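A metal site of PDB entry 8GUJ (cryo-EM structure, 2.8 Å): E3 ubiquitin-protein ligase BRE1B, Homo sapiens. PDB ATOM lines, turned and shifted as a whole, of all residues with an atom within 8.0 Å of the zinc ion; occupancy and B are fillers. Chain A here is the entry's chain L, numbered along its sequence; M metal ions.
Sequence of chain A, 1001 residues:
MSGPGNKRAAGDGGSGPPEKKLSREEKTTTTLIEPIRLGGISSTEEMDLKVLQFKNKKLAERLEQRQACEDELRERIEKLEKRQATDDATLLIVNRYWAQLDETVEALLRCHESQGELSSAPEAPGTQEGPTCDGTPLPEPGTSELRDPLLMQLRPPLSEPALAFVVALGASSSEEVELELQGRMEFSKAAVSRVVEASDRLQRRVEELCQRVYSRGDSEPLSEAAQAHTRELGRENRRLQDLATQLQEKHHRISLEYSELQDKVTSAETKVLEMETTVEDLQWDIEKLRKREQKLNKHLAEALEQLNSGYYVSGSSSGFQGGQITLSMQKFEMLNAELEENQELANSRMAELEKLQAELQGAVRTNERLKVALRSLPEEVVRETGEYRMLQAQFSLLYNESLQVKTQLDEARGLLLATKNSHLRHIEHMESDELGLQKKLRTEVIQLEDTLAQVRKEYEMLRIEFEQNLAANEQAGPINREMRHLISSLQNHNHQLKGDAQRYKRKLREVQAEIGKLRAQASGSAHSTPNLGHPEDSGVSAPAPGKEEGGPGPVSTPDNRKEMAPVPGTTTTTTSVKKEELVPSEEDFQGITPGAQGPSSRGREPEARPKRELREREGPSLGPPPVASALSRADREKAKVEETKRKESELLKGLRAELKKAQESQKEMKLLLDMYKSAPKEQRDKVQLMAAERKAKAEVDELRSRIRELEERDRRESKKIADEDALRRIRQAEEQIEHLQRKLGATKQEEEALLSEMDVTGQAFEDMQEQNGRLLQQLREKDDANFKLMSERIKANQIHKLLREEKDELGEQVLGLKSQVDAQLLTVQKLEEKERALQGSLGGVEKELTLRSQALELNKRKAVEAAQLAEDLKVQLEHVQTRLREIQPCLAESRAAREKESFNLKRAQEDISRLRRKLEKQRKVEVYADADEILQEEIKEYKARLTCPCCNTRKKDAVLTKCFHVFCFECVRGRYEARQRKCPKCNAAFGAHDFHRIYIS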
ATOM      1  N   THR A 947     -16.962 -13.987   9.982  1.00  0.00           N
ATOM      2  CA  THR A 947     -17.287 -12.569  10.099  1.00  0.00           C
ATOM      3  C   THR A 947     -16.923 -12.077  11.495  1.00  0.00           C
ATOM      4  O   THR A 947     -17.085 -12.810  12.477  1.00  0.00           O
ATOM      5  CB  THR A 947     -18.781 -12.338   9.830  1.00  0.00           C
ATOM      6  OG1 THR A 947     -19.169 -13.064   8.658  1.00  0.00           O
ATOM      7  CG2 THR A 947     -19.048 -10.878   9.582  1.00  0.00           C
ATOM      8  N   CYS A 948     -16.417 -10.851  11.568  1.00  0.00           N
ATOM      9  CA  CYS A 948     -15.936 -10.251  12.818  1.00  0.00           C
ATOM     10  C   CYS A 948     -17.059 -10.128  13.844  1.00  0.00           C
ATOM     11  O   CYS A 948     -18.104  -9.544  13.536  1.00  0.00           O
ATOM     12  CB  CYS A 948     -15.337  -8.877  12.500  1.00  0.00           C
ATOM     13  SG  CYS A 948     -14.786  -7.863  13.903  1.00  0.00           S
ATOM     14  N   PRO A 949     -16.896 -10.680  15.059  1.00  0.00           N
ATOM     15  CA  PRO A 949     -17.952 -10.558  16.068  1.00  0.00           C
ATOM     16  C   PRO A 949     -18.309  -9.117  16.395  1.00  0.00           C
ATOM     17  O   PRO A 949     -19.480  -8.842  16.707  1.00  0.00           O
ATOM     18  CB  PRO A 949     -17.337 -11.244  17.292  1.00  0.00           C
ATOM     19  CG  PRO A 949     -16.289 -12.180  16.752  1.00  0.00           C
ATOM     20  CD  PRO A 949     -16.096 -11.896  15.284  1.00  0.00           C
ATOM     21  N   CYS A 950     -17.346  -8.209  16.347  1.00  0.00           N
ATOM     22  CA  CYS A 950     -17.638  -6.803  16.629  1.00  0.00           C
ATOM     23  C   CYS A 950     -18.541  -6.191  15.579  1.00  0.00           C
ATOM     24  O   CYS A 950     -19.408  -5.373  15.904  1.00  0.00           O
ATOM     25  CB  CYS A 950     -16.330  -6.005  16.751  1.00  0.00           C
ATOM     26  SG  CYS A 950     -16.567  -4.254  17.126  1.00  0.00           S
ATOM     27  N   CYS A 951     -18.367  -6.569  14.312  1.00  0.00           N
ATOM     28  CA  CYS A 951     -19.138  -5.981  13.219  1.00  0.00           C
ATOM     29  C   CYS A 951     -20.276  -6.853  12.729  1.00  0.00           C
ATOM     30  O   CYS A 951     -21.397  -6.359  12.580  1.00  0.00           O
ATOM     31  CB  CYS A 951     -18.206  -5.652  12.034  1.00  0.00           C
ATOM     32  SG  CYS A 951     -17.254  -7.038  11.381  1.00  0.00           S
ATOM     33  N   ASN A 952     -20.016  -8.147  12.482  1.00  0.00           N
ATOM     34  CA  ASN A 952     -21.023  -9.086  11.987  1.00  0.00           C
ATOM     35  C   ASN A 952     -21.670  -8.595  10.687  1.00  0.00           C
ATOM     36  O   ASN A 952     -22.875  -8.778  10.479  1.00  0.00           O
ATOM     37  CB  ASN A 952     -22.086  -9.380  13.042  1.00  0.00           C
ATOM     38  CG  ASN A 952     -21.553 -10.223  14.185  1.00  0.00           C
ATOM     39  OD1 ASN A 952     -20.942 -11.273  13.954  1.00  0.00           O
ATOM     40  ND2 ASN A 952     -21.773  -9.775  15.412  1.00  0.00           N
ATOM     41  N   THR A 953     -20.879  -7.976   9.822  1.00  0.00           N
ATOM     42  CA  THR A 953     -21.389  -7.435   8.564  1.00  0.00           C
ATOM     43  C   THR A 953     -20.519  -7.890   7.400  1.00  0.00           C
ATOM     44  O   THR A 953     -21.004  -8.077   6.285  1.00  0.00           O
ATOM     45  CB  THR A 953     -21.452  -5.902   8.652  1.00  0.00           C
ATOM     46  OG1 THR A 953     -22.282  -5.509   9.744  1.00  0.00           O
ATOM     47  CG2 THR A 953     -22.028  -5.304   7.371  1.00  0.00           C
ATOM     48  N   ARG A 954     -19.236  -8.093   7.681  1.00  0.00           N
ATOM     49  CA  ARG A 954     -18.229  -8.316   6.649  1.00  0.00           C
ATOM     50  C   ARG A 954     -16.988  -8.948   7.268  1.00  0.00           C
ATOM     51  O   ARG A 954     -16.764  -8.885   8.478  1.00  0.00           O
ATOM     52  CB  ARG A 954     -17.911  -7.035   5.862  1.00  0.00           C
ATOM     53  CG  ARG A 954     -16.965  -6.042   6.508  1.00  0.00           C
ATOM     54  CD  ARG A 954     -17.663  -5.435   7.712  1.00  0.00           C
ATOM     55  NE  ARG A 954     -16.915  -4.404   8.417  1.00  0.00           N
ATOM     56  CZ  ARG A 954     -16.015  -4.685   9.346  1.00  0.00           C
ATOM     57  NH1 ARG A 954     -15.663  -5.921   9.621  1.00  0.00           N
ATOM     58  NH2 ARG A 954     -15.457  -3.678  10.016  1.00  0.00           N
ATOM     59  N   LYS A 955     -16.171  -9.531   6.397  1.00  0.00           N
ATOM     60  CA  LYS A 955     -15.277 -10.644   6.727  1.00  0.00           C
ATOM     61  C   LYS A 955     -14.017 -10.204   7.454  1.00  0.00           C
ATOM     62  O   LYS A 955     -13.495  -9.108   7.251  1.00  0.00           O
ATOM     63  CB  LYS A 955     -14.929 -11.380   5.423  1.00  0.00           C
ATOM     64  CG  LYS A 955     -14.143 -12.664   5.557  1.00  0.00           C
ATOM     65  CD  LYS A 955     -12.750 -12.452   5.020  1.00  0.00           C
ATOM     66  CE  LYS A 955     -12.753 -12.277   3.518  1.00  0.00           C
ATOM     67  NZ  LYS A 955     -11.386 -12.069   2.972  1.00  0.00           N
ATOM     68  N   LYS A 956     -13.523 -11.092   8.320  1.00  0.00           N
ATOM     69  CA  LYS A 956     -12.317 -10.851   9.114  1.00  0.00           C
ATOM     70  C   LYS A 956     -11.078 -10.790   8.231  1.00  0.00           C
ATOM     71  O   LYS A 956     -10.888 -11.640   7.363  1.00  0.00           O
ATOM     72  CB  LYS A 956     -12.121 -11.961  10.142  1.00  0.00           C
ATOM     73  CG  LYS A 956     -13.267 -12.237  11.086  1.00  0.00           C
ATOM     74  CD  LYS A 956     -12.866 -13.360  12.032  1.00  0.00           C
ATOM     75  CE  LYS A 956     -13.925 -13.656  13.077  1.00  0.00           C
ATOM     76  NZ  LYS A 956     -15.089 -14.361  12.485  1.00  0.00           N
ATOM     77  N   ASP A 957     -10.200  -9.815   8.486  1.00  0.00           N
ATOM     78  CA  ASP A 957      -8.909  -9.827   7.818  1.00  0.00           C
ATOM     79  C   ASP A 957      -7.731  -9.368   8.706  1.00  0.00           C
ATOM     80  O   ASP A 957      -6.703  -8.937   8.167  1.00  0.00           O
ATOM     81  CB  ASP A 957      -9.019  -9.053   6.467  1.00  0.00           C
ATOM     82  CG  ASP A 957      -8.852  -7.532   6.589  1.00  0.00           C
ATOM     83  OD1 ASP A 957      -8.625  -6.974   7.675  1.00  0.00           O
ATOM     84  OD2 ASP A 957      -8.932  -6.876   5.529  1.00  0.00           O
ATOM     85  N   VAL A 966      -8.870 -13.514  15.603  1.00  0.00           N
ATOM     86  CA  VAL A 966      -8.985 -12.922  14.281  1.00  0.00           C
ATOM     87  C   VAL A 966     -10.179 -11.980  14.234  1.00  0.00           C
ATOM     88  O   VAL A 966     -11.290 -12.342  14.665  1.00  0.00           O
ATOM     89  CB  VAL A 966      -9.112 -14.016  13.193  1.00  0.00           C
ATOM     90  CG1 VAL A 966      -8.980 -13.395  11.808  1.00  0.00           C
ATOM     91  CG2 VAL A 966      -8.063 -15.067  13.387  1.00  0.00           C
ATOM     92  N   PHE A 967      -9.941 -10.769  13.753  1.00  0.00           N
ATOM     93  CA  PHE A 967     -11.002  -9.792  13.513  1.00  0.00           C
ATOM     94  C   PHE A 967     -10.737  -9.178  12.136  1.00  0.00           C
ATOM     95  O   PHE A 967      -9.996  -9.719  11.317  1.00  0.00           O
ATOM     96  CB  PHE A 967     -11.075  -8.720  14.616  1.00  0.00           C
ATOM     97  CG  PHE A 967     -11.400  -9.272  15.992  1.00  0.00           C
ATOM     98  CD1 PHE A 967     -10.463  -9.984  16.725  1.00  0.00           C
ATOM     99  CD2 PHE A 967     -12.653  -9.066  16.533  1.00  0.00           C
ATOM    100  CE1 PHE A 967     -10.776 -10.488  17.968  1.00  0.00           C
ATOM    101  CE2 PHE A 967     -12.969  -9.568  17.786  1.00  0.00           C
ATOM    102  CZ  PHE A 967     -12.032 -10.277  18.497  1.00  0.00           C
ATOM    103  N   CYS A 968     -11.381  -8.056  11.867  1.00  0.00           N
ATOM    104  CA  CYS A 968     -11.201  -7.303  10.641  1.00  0.00           C
ATOM    105  C   CYS A 968     -10.456  -6.004  10.932  1.00  0.00           C
ATOM    106  O   CYS A 968     -10.495  -5.495  12.055  1.00  0.00           O
ATOM    107  CB  CYS A 968     -12.535  -7.006   9.989  1.00  0.00           C
ATOM    108  SG  CYS A 968     -13.405  -5.762  10.902  1.00  0.00           S
ATOM    109  N   PHE A 969      -9.752  -5.488   9.921  1.00  0.00           N
ATOM    110  CA  PHE A 969      -8.772  -4.426  10.157  1.00  0.00           C
ATOM    111  C   PHE A 969      -9.435  -3.113  10.574  1.00  0.00           C
ATOM    112  O   PHE A 969      -8.968  -2.457  11.506  1.00  0.00           O
ATOM    113  CB  PHE A 969      -7.921  -4.216   8.896  1.00  0.00           C
ATOM    114  CG  PHE A 969      -6.856  -3.172   9.048  1.00  0.00           C
ATOM    115  CD1 PHE A 969      -5.707  -3.444   9.766  1.00  0.00           C
ATOM    116  CD2 PHE A 969      -6.992  -1.937   8.444  1.00  0.00           C
ATOM    117  CE1 PHE A 969      -4.717  -2.493   9.905  1.00  0.00           C
ATOM    118  CE2 PHE A 969      -6.005  -0.981   8.570  1.00  0.00           C
ATOM    119  CZ  PHE A 969      -4.870  -1.258   9.305  1.00  0.00           C
ATOM    120  N   GLU A 970     -10.514  -2.708   9.893  1.00  0.00           N
ATOM    121  CA  GLU A 970     -11.012  -1.375  10.141  1.00  0.00           C
ATOM    122  C   GLU A 970     -11.874  -1.318  11.408  1.00  0.00           C
ATOM    123  O   GLU A 970     -12.025  -0.252  11.994  1.00  0.00           O
ATOM    124  CB  GLU A 970     -11.764  -0.810   8.918  1.00  0.00           C
ATOM    125  CG  GLU A 970     -13.000  -1.513   8.439  1.00  0.00           C
ATOM    126  CD  GLU A 970     -14.219  -1.024   9.173  1.00  0.00           C
ATOM    127  OE1 GLU A 970     -14.151   0.069   9.773  1.00  0.00           O
ATOM    128  OE2 GLU A 970     -15.260  -1.681   9.084  1.00  0.00           O
ATOM    129  N   CYS A 971     -12.419  -2.456  11.857  1.00  0.00           N
ATOM    130  CA  CYS A 971     -13.083  -2.475  13.168  1.00  0.00           C
ATOM    131  C   CYS A 971     -12.093  -2.183  14.294  1.00  0.00           C
ATOM    132  O   CYS A 971     -12.358  -1.349  15.168  1.00  0.00           O
ATOM    133  CB  CYS A 971     -13.777  -3.815  13.422  1.00  0.00           C
ATOM    134  SG  CYS A 971     -15.467  -4.007  12.783  1.00  0.00           S
ATOM    135  N   VAL A 972     -10.944  -2.875  14.303  1.00  0.00           N
ATOM    136  CA  VAL A 972      -9.969  -2.598  15.350  1.00  0.00           C
ATOM    137  C   VAL A 972      -9.334  -1.230  15.145  1.00  0.00           C
ATOM    138  O   VAL A 972      -8.961  -0.569  16.127  1.00  0.00           O
ATOM    139  CB  VAL A 972      -8.909  -3.723  15.452  1.00  0.00           C
ATOM    140  CG1 VAL A 972      -9.554  -5.018  15.934  1.00  0.00           C
ATOM    141  CG2 VAL A 972      -8.206  -3.942  14.132  1.00  0.00           C
ATOM    142  N   ARG A 975     -11.805   1.009  16.790  1.00  0.00           N
ATOM    143  CA  ARG A 975     -11.721   0.892  18.237  1.00  0.00           C
ATOM    144  C   ARG A 975     -10.490   1.615  18.787  1.00  0.00           C
ATOM    145  O   ARG A 975     -10.572   2.274  19.836  1.00  0.00           O
ATOM    146  CB  ARG A 975     -11.696  -0.577  18.655  1.00  0.00           C
ATOM    147  CG  ARG A 975     -13.009  -1.316  18.423  1.00  0.00           C
ATOM    148  CD  ARG A 975     -12.823  -2.817  18.593  1.00  0.00           C
ATOM    149  NE  ARG A 975     -12.692  -3.198  19.994  1.00  0.00           N
ATOM    150  CZ  ARG A 975     -13.689  -3.235  20.868  1.00  0.00           C
ATOM    151  NH1 ARG A 975     -14.926  -2.929  20.511  1.00  0.00           N
ATOM    152  NH2 ARG A 975     -13.442  -3.588  22.124  1.00  0.00           N
ATOM    153  N   PRO A 984     -12.685  -7.117  21.497  1.00  0.00           N
ATOM    154  CA  PRO A 984     -14.152  -7.174  21.645  1.00  0.00           C
ATOM    155  C   PRO A 984     -14.665  -8.392  22.390  1.00  0.00           C
ATOM    156  O   PRO A 984     -15.774  -8.330  22.935  1.00  0.00           O
ATOM    157  CB  PRO A 984     -14.637  -7.157  20.192  1.00  0.00           C
ATOM    158  CG  PRO A 984     -13.564  -6.460  19.442  1.00  0.00           C
ATOM    159  CD  PRO A 984     -12.273  -6.842  20.114  1.00  0.00           C
HETATM  160 ZN    ZN M   1     -15.234  -6.266  12.264  1.00  0.00          ZN
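Within 4 Å of the zinc ion: Cys 948, Cys 951, Arg 954, Cys 968 and Cys 971.
O of Cys 948 lies close to OD1 of Asn 952, at 3.3 Å.
SG of Cys 948 lies close to N of Cys 950 (3.6 Å).
The side-chain sulfur (SG) of Cys 971 lies close to the guanidinium group (NH2) of Arg 954 (2.8 Å).
NE of Arg 954 is in salt-bridge range of OE2 of Glu 970 (3.3 Å).
The side-chain sulfur of Cys 951 sits close to the guanidinium group of Arg 954 (2.6 Å).
The side-chain sulfur (SG) of Cys 968 sits close to the guanidinium group (NH1) of Arg 954 (2.6 Å).
O of Cys 951 sits at hydrogen-bond distance from OG1 of Thr 953.
The zinc ion is bound by the side-chain sulfur (SG) of Cys 971 (2.3 Å), the side-chain sulfur (SG) of Cys 948 (2.3 Å), the side-chain sulfur (SG) of Cys 968 (2.3 Å) and the side-chain sulfur (SG) of Cys 951 (2.3 Å).
The zinc ion has four donor atoms within binding distance.
Slightly farther from the zinc ion lies NH1 of Arg 954 (2.7 Å).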
